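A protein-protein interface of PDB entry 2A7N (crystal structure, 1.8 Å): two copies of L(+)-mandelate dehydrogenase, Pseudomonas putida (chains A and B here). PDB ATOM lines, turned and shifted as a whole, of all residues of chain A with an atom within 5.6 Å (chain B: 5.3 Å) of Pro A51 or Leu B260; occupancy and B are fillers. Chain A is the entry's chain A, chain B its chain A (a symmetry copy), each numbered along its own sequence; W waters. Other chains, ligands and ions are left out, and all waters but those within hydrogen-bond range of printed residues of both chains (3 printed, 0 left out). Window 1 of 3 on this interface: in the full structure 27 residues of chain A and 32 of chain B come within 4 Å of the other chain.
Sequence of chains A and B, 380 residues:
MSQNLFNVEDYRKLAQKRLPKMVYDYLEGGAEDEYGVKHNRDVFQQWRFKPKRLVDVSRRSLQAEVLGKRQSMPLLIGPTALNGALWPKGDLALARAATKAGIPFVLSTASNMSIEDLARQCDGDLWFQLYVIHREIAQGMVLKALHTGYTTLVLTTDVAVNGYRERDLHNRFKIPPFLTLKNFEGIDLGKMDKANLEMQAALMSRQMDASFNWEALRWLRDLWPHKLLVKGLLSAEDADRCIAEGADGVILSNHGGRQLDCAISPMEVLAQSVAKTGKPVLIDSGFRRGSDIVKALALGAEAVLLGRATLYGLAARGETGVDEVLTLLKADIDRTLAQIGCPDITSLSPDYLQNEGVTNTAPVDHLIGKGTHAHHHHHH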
ATOM      1  N   PHE A  49      23.818   3.685  19.423  1.00  0.00           N
ATOM      2  CA  PHE A  49      24.158   3.407  20.810  1.00  0.00           C
ATOM      3  C   PHE A  49      23.641   2.095  21.378  1.00  0.00           C
ATOM      4  O   PHE A  49      22.547   1.639  21.040  1.00  0.00           O
ATOM      5  CB  PHE A  49      23.642   4.530  21.714  1.00  0.00           C
ATOM      6  CG  PHE A  49      24.295   5.858  21.475  1.00  0.00           C
ATOM      7  CD1 PHE A  49      25.677   5.996  21.559  1.00  0.00           C
ATOM      8  CD2 PHE A  49      23.520   6.985  21.220  1.00  0.00           C
ATOM      9  CE1 PHE A  49      26.278   7.238  21.388  1.00  0.00           C
ATOM     10  CE2 PHE A  49      24.112   8.233  21.050  1.00  0.00           C
ATOM     11  CZ  PHE A  49      25.495   8.360  21.138  1.00  0.00           C
ATOM     12  N   LYS A  50      24.452   1.506  22.253  1.00  0.00           N
ATOM     13  CA  LYS A  50      24.105   0.289  22.974  1.00  0.00           C
ATOM     14  C   LYS A  50      24.313   0.678  24.434  1.00  0.00           C
ATOM     15  O   LYS A  50      25.395   0.498  24.993  1.00  0.00           O
ATOM     16  CB  LYS A  50      25.025  -0.882  22.598  1.00  0.00           C
ATOM     17  CG  LYS A  50      24.810  -1.392  21.183  1.00  0.00           C
ATOM     18  CD  LYS A  50      25.661  -2.620  20.874  1.00  0.00           C
ATOM     19  CE  LYS A  50      25.214  -3.834  21.669  1.00  0.00           C
ATOM     20  NZ  LYS A  50      25.903  -5.070  21.180  1.00  0.00           N
ATOM     21  N   PRO A  51      23.277   1.263  25.055  1.00  0.00           N
ATOM     22  CA  PRO A  51      23.307   1.703  26.453  1.00  0.00           C
ATOM     23  C   PRO A  51      23.628   0.588  27.444  1.00  0.00           C
ATOM     24  O   PRO A  51      23.338  -0.583  27.193  1.00  0.00           O
ATOM     25  CB  PRO A  51      21.895   2.248  26.675  1.00  0.00           C
ATOM     26  CG  PRO A  51      21.491   2.729  25.322  1.00  0.00           C
ATOM     27  CD  PRO A  51      22.000   1.631  24.418  1.00  0.00           C
ATOM     28  N   LYS A  52      24.235   0.971  28.564  1.00  0.00           N
ATOM     29  CA  LYS A  52      24.556   0.044  29.643  1.00  0.00           C
ATOM     30  C   LYS A  52      23.543   0.396  30.726  1.00  0.00           C
ATOM     31  O   LYS A  52      23.603   1.478  31.311  1.00  0.00           O
ATOM     32  CB  LYS A  52      25.979   0.272  30.157  1.00  0.00           C
ATOM     33  CG  LYS A  52      27.057   0.015  29.113  1.00  0.00           C
ATOM     34  CD  LYS A  52      28.454   0.098  29.719  1.00  0.00           C
ATOM     35  CE  LYS A  52      29.530  -0.097  28.658  1.00  0.00           C
ATOM     36  NZ  LYS A  52      29.339  -1.365  27.897  1.00  0.00           N
ATOM     37  N   ARG A  53      22.598  -0.506  30.968  1.00  0.00           N
ATOM     38  CA  ARG A  53      21.551  -0.270  31.949  1.00  0.00           C
ATOM     39  C   ARG A  53      21.945  -0.568  33.392  1.00  0.00           C
ATOM     40  O   ARG A  53      22.963  -1.207  33.659  1.00  0.00           O
ATOM     41  CB  ARG A  53      20.305  -1.089  31.591  1.00  0.00           C
ATOM     42  CG  ARG A  53      19.650  -0.704  30.268  1.00  0.00           C
ATOM     43  CD  ARG A  53      19.168   0.735  30.276  1.00  0.00           C
ATOM     44  NE  ARG A  53      18.638   1.128  28.974  1.00  0.00           N
ATOM     45  CZ  ARG A  53      18.772   2.344  28.457  1.00  0.00           C
ATOM     46  NH1 ARG A  53      19.412   3.287  29.134  1.00  0.00           N
ATOM     47  NH2 ARG A  53      18.287   2.612  27.253  1.00  0.00           N
ATOM     48  N   THR A 336      22.644  12.539  27.145  1.00  0.00           N
ATOM     49  CA  THR A 336      23.105  11.388  26.383  1.00  0.00           C
ATOM     50  C   THR A 336      23.954  10.457  27.246  1.00  0.00           C
ATOM     51  O   THR A 336      23.804   9.235  27.188  1.00  0.00           O
ATOM     52  CB  THR A 336      23.903  11.847  25.147  1.00  0.00           C
ATOM     53  OG1 THR A 336      23.055  12.647  24.313  1.00  0.00           O
ATOM     54  CG2 THR A 336      24.399  10.649  24.343  1.00  0.00           C
ATOM     55  N   GLN A 339      21.649   8.477  29.483  1.00  0.00           N
ATOM     56  CA  GLN A 339      20.908   7.459  28.748  1.00  0.00           C
ATOM     57  C   GLN A 339      21.732   6.250  28.300  1.00  0.00           C
ATOM     58  O   GLN A 339      21.190   5.154  28.180  1.00  0.00           O
ATOM     59  CB  GLN A 339      20.213   8.097  27.542  1.00  0.00           C
ATOM     60  CG  GLN A 339      19.075   9.075  27.902  1.00  0.00           C
ATOM     61  CD  GLN A 339      17.762   8.383  28.259  1.00  0.00           C
ATOM     62  OE1 GLN A 339      16.767   9.044  28.582  1.00  0.00           O
ATOM     63  NE2 GLN A 339      17.747   7.055  28.197  1.00  0.00           N
ATOM     64  N   ILE A 340      23.027   6.429  28.040  1.00  0.00           N
ATOM     65  CA  ILE A 340      23.839   5.287  27.622  1.00  0.00           C
ATOM     66  C   ILE A 340      24.536   4.621  28.808  1.00  0.00           C
ATOM     67  O   ILE A 340      25.226   3.616  28.651  1.00  0.00           O
ATOM     68  CB  ILE A 340      24.896   5.675  26.550  1.00  0.00           C
ATOM     69  CG1 ILE A 340      25.920   6.651  27.131  1.00  0.00           C
ATOM     70  CG2 ILE A 340      24.191   6.262  25.325  1.00  0.00           C
ATOM     71  CD1 ILE A 340      27.054   7.003  26.170  1.00  0.00           C
ATOM     72  N   GLY A 341      24.341   5.181  29.997  1.00  0.00           N
ATOM     73  CA  GLY A 341      24.941   4.612  31.192  1.00  0.00           C
ATOM     74  C   GLY A 341      26.416   4.891  31.421  1.00  0.00           C
ATOM     75  O   GLY A 341      27.117   4.062  32.005  1.00  0.00           O
ATOM     76  N   TYR A 352      30.191   1.377  23.781  1.00  0.00           N
ATOM     77  CA  TYR A 352      28.837   1.929  23.828  1.00  0.00           C
ATOM     78  C   TYR A 352      28.258   2.100  22.427  1.00  0.00           C
ATOM     79  O   TYR A 352      27.116   2.535  22.271  1.00  0.00           O
ATOM     80  CB  TYR A 352      28.834   3.297  24.518  1.00  0.00           C
ATOM     81  CG  TYR A 352      29.253   3.272  25.966  1.00  0.00           C
ATOM     82  CD1 TYR A 352      30.600   3.245  26.327  1.00  0.00           C
ATOM     83  CD2 TYR A 352      28.296   3.272  26.981  1.00  0.00           C
ATOM     84  CE1 TYR A 352      30.986   3.221  27.667  1.00  0.00           C
ATOM     85  CE2 TYR A 352      28.668   3.247  28.320  1.00  0.00           C
ATOM     86  CZ  TYR A 352      30.009   3.221  28.657  1.00  0.00           C
ATOM     87  OH  TYR A 352      30.363   3.191  29.982  1.00  0.00           O
ATOM     88  N   ALA B  31      12.214  10.778  20.322  1.00  0.00           N
ATOM     89  CA  ALA B  31      13.283  11.646  20.795  1.00  0.00           C
ATOM     90  C   ALA B  31      13.975  12.392  19.655  1.00  0.00           C
ATOM     91  O   ALA B  31      14.160  11.858  18.561  1.00  0.00           O
ATOM     92  CB  ALA B  31      14.308  10.827  21.580  1.00  0.00           C
ATOM     93  N   LEU B 234      19.329  -3.257  25.827  1.00  0.00           N
ATOM     94  CA  LEU B 234      19.751  -3.183  24.433  1.00  0.00           C
ATOM     95  C   LEU B 234      21.101  -3.851  24.173  1.00  0.00           C
ATOM     96  O   LEU B 234      21.884  -3.389  23.348  1.00  0.00           O
ATOM     97  CB  LEU B 234      19.792  -1.720  23.976  1.00  0.00           C
ATOM     98  CG  LEU B 234      18.418  -1.051  23.854  1.00  0.00           C
ATOM     99  CD1 LEU B 234      18.578   0.458  23.717  1.00  0.00           C
ATOM    100  CD2 LEU B 234      17.673  -1.630  22.658  1.00  0.00           C
ATOM    101  N   SER B 235      21.376  -4.932  24.895  1.00  0.00           N
ATOM    102  CA  SER B 235      22.612  -5.684  24.699  1.00  0.00           C
ATOM    103  C   SER B 235      22.458  -7.053  25.334  1.00  0.00           C
ATOM    104  O   SER B 235      21.790  -7.199  26.362  1.00  0.00           O
ATOM    105  CB  SER B 235      23.819  -4.968  25.320  1.00  0.00           C
ATOM    106  OG  SER B 235      23.858  -5.135  26.727  1.00  0.00           O
ATOM    107  N   ASP B 238      23.870  -7.094  28.945  1.00  0.00           N
ATOM    108  CA  ASP B 238      22.996  -6.618  30.014  1.00  0.00           C
ATOM    109  C   ASP B 238      21.903  -7.640  30.291  1.00  0.00           C
ATOM    110  O   ASP B 238      21.541  -7.876  31.442  1.00  0.00           O
ATOM    111  CB  ASP B 238      22.354  -5.269  29.657  1.00  0.00           C
ATOM    112  CG  ASP B 238      23.233  -4.083  30.028  1.00  0.00           C
ATOM    113  OD1 ASP B 238      24.272  -4.291  30.693  1.00  0.00           O
ATOM    114  OD2 ASP B 238      22.882  -2.942  29.659  1.00  0.00           O
ATOM    115  N   ASN B 254      13.834  -0.091  23.228  1.00  0.00           N
ATOM    116  CA  ASN B 254      14.420   1.245  23.242  1.00  0.00           C
ATOM    117  C   ASN B 254      13.293   2.238  23.525  1.00  0.00           C
ATOM    118  O   ASN B 254      13.333   3.402  23.127  1.00  0.00           O
ATOM    119  CB  ASN B 254      15.187   1.606  21.947  1.00  0.00           C
ATOM    120  CG  ASN B 254      14.327   1.581  20.692  1.00  0.00           C
ATOM    121  OD1 ASN B 254      13.137   1.888  20.720  1.00  0.00           O
ATOM    122  ND2 ASN B 254      14.953   1.237  19.565  1.00  0.00           N
ATOM    123  N   GLY B 257      11.546   4.304  20.713  1.00  0.00           N
ATOM    124  CA  GLY B 257      12.295   5.438  20.187  1.00  0.00           C
ATOM    125  C   GLY B 257      12.017   6.761  20.882  1.00  0.00           C
ATOM    126  O   GLY B 257      12.277   7.829  20.324  1.00  0.00           O
ATOM    127  N   ARG B 258      11.516   6.699  22.112  1.00  0.00           N
ATOM    128  CA  ARG B 258      11.170   7.904  22.858  1.00  0.00           C
ATOM    129  C   ARG B 258      12.223   8.406  23.849  1.00  0.00           C
ATOM    130  O   ARG B 258      12.056   9.479  24.433  1.00  0.00           O
ATOM    131  CB  ARG B 258       9.848   7.668  23.598  1.00  0.00           C
ATOM    132  CG  ARG B 258       8.670   7.389  22.669  1.00  0.00           C
ATOM    133  CD  ARG B 258       7.520   6.723  23.411  1.00  0.00           C
ATOM    134  NE  ARG B 258       6.860   7.590  24.389  1.00  0.00           N
ATOM    135  CZ  ARG B 258       5.995   8.555  24.084  1.00  0.00           C
ATOM    136  NH1 ARG B 258       5.672   8.800  22.818  1.00  0.00           N
ATOM    137  NH2 ARG B 258       5.424   9.258  25.052  1.00  0.00           N
ATOM    138  N   GLN B 259      13.304   7.653  24.029  1.00  0.00           N
ATOM    139  CA  GLN B 259      14.336   8.038  24.990  1.00  0.00           C
ATOM    140  C   GLN B 259      15.690   8.464  24.429  1.00  0.00           C
ATOM    141  O   GLN B 259      16.260   9.465  24.865  1.00  0.00           O
ATOM    142  CB  GLN B 259      14.546   6.898  25.993  1.00  0.00           C
ATOM    143  CG  GLN B 259      13.408   6.749  26.985  1.00  0.00           C
ATOM    144  CD  GLN B 259      13.316   7.943  27.917  1.00  0.00           C
ATOM    145  OE1 GLN B 259      14.164   8.131  28.791  1.00  0.00           O
ATOM    146  NE2 GLN B 259      12.297   8.764  27.722  1.00  0.00           N
ATOM    147  N   LEU B 260      16.206   7.703  23.473  1.00  0.00           N
ATOM    148  CA  LEU B 260      17.507   7.992  22.879  1.00  0.00           C
ATOM    149  C   LEU B 260      17.348   7.780  21.381  1.00  0.00           C
ATOM    150  O   LEU B 260      17.234   6.646  20.920  1.00  0.00           O
ATOM    151  CB  LEU B 260      18.557   7.035  23.457  1.00  0.00           C
ATOM    152  CG  LEU B 260      20.016   7.176  23.020  1.00  0.00           C
ATOM    153  CD1 LEU B 260      20.526   8.579  23.377  1.00  0.00           C
ATOM    154  CD2 LEU B 260      20.860   6.105  23.711  1.00  0.00           C
ATOM    155  N   ASP B 261      17.345   8.872  20.623  1.00  0.00           N
ATOM    156  CA  ASP B 261      17.136   8.783  19.185  1.00  0.00           C
ATOM    157  C   ASP B 261      18.081   7.850  18.437  1.00  0.00           C
ATOM    158  O   ASP B 261      17.654   7.159  17.511  1.00  0.00           O
ATOM    159  CB  ASP B 261      17.176  10.181  18.554  1.00  0.00           C
ATOM    160  CG  ASP B 261      16.479  10.229  17.201  1.00  0.00           C
ATOM    161  OD1 ASP B 261      15.430   9.559  17.046  1.00  0.00           O
ATOM    162  OD2 ASP B 261      16.967  10.944  16.297  1.00  0.00           O
ATOM    163  N   CYS B 262      19.348   7.807  18.835  1.00  0.00           N
ATOM    164  CA  CYS B 262      20.315   6.957  18.141  1.00  0.00           C
ATOM    165  C   CYS B 262      20.557   5.580  18.757  1.00  0.00           C
ATOM    166  O   CYS B 262      21.555   4.921  18.451  1.00  0.00           O
ATOM    167  CB  CYS B 262      21.645   7.699  17.997  1.00  0.00           C
ATOM    168  SG  CYS B 262      21.501   9.283  17.132  1.00  0.00           S
ATOM    169  N   ALA B 263      19.655   5.142  19.628  1.00  0.00           N
ATOM    170  CA  ALA B 263      19.791   3.819  20.229  1.00  0.00           C
ATOM    171  C   ALA B 263      19.573   2.789  19.128  1.00  0.00           C
ATOM    172  O   ALA B 263      18.862   3.052  18.154  1.00  0.00           O
ATOM    173  CB  ALA B 263      18.745   3.623  21.325  1.00  0.00           C
HETATM  174  O   HOH W   1      25.054  -2.266  32.347  1.00  0.00           O
HETATM  175  O   HOH W   2      21.345  -2.288  27.674  1.00  0.00           O
HETATM  176  O   HOH W   3      24.922  -2.806  27.340  1.00  0.00           O
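The backbone NH of Lys A50 sits at hydrogen-bond distance from the backbone carbonyl oxygen of Tyr A352, 2.9 Å away.
The backbone NH of Lys A52 is in hydrogen-bond range of the backbone carbonyl oxygen of Ile A340 (2.8 Å).
O of Gln A339 sits at hydrogen-bond distance from NH1 of Arg A53 (2.7 Å).
OG of Ser B235 sits at hydrogen-bond distance from N of Asp B238, 3.0 Å away.
Among the printed residues, pairs that only touch across the chains: Lys A52 with Asp B238, Phe A49 with Ala B263, Pro A51 with Leu B234, Ile A340 with Leu B260, Phe A49 with Leu B260, Lys A50 with Leu B234 and Pro A51 with Leu B260.
Leu B260 touches just these residues of chain A: Phe A49 (3.7 Å), Pro A51 (3.8 Å) and Ile A340 (3.7 Å).
Printed residues of chain A within 4 Å of Cys B262: Phe A49 (2.8 Å).
Of the printed residues of chain A, Asp B238 touches Pro A51, Lys A52 and Arg A53.
Printed residues of chain B within 4 Å of Phe A49: Leu B260, Cys B262 and Ala B263.
Of the printed residues of chain B, Ile A340 touches Leu B260.
Printed residues of chain A within 4 Å of Leu B234: Lys A50 (3.8 Å) and Pro A51 (3.7 Å).
Asn B254 touches none of the printed residues of chain A.
Ala B31 touches none of the printed residues of chain A.
Water W2 lies within hydrogen-bond range of OD2 of Asp B238 (2.6 Å), O of Pro A51 (2.7 Å) and N of Leu B234 (2.9 Å).
Water W3 lies within hydrogen-bond range of OG of Ser B235 (2.6 Å), O of Pro A51 (2.7 Å) and OD2 of Asp B238 (3.1 Å).
Water W1 bridges the backbone carbonyl oxygen of Arg A53 (2.7 Å) and the side-chain carboxylate of Asp B238 (2.7 Å).
Printed residues of chain B that touch a printed residue of chain A: Leu B234, Asp B238, Gln B259, Leu B260, Cys B262 and Ala B263.
Along chain A the printed residues that touch a printed residue of chain B span positions 49 to 340.
Among the printed residues, 11 pairs touch across the chains.
Among the printed residues, no Asp or Glu carboxylate lies within 4 Å of a Lys or Arg side-chain nitrogen of the other chain.
No position is printed for both chains.
Of the 11 pairs that touch across the chains among the printed residues, none has its exchanged pair printed and touching as well.
The backbone carbonyl oxygen of Cys B262 sits at hydrogen-bond distance from the backbone NH of Phe A49 (2.8 Å).
The side-chain carboxylate of Asp B238 is in hydrogen-bond range of the backbone NH of Arg A53 (2.8 Å).
The side-chain amide oxygen (OE1) of Gln A339 sits close to the side-chain amide oxygen (OE1) of Gln B259, at 2.8 Å.
OD2 of Asp B238 sits close to O of Pro A51 (3.4 Å).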
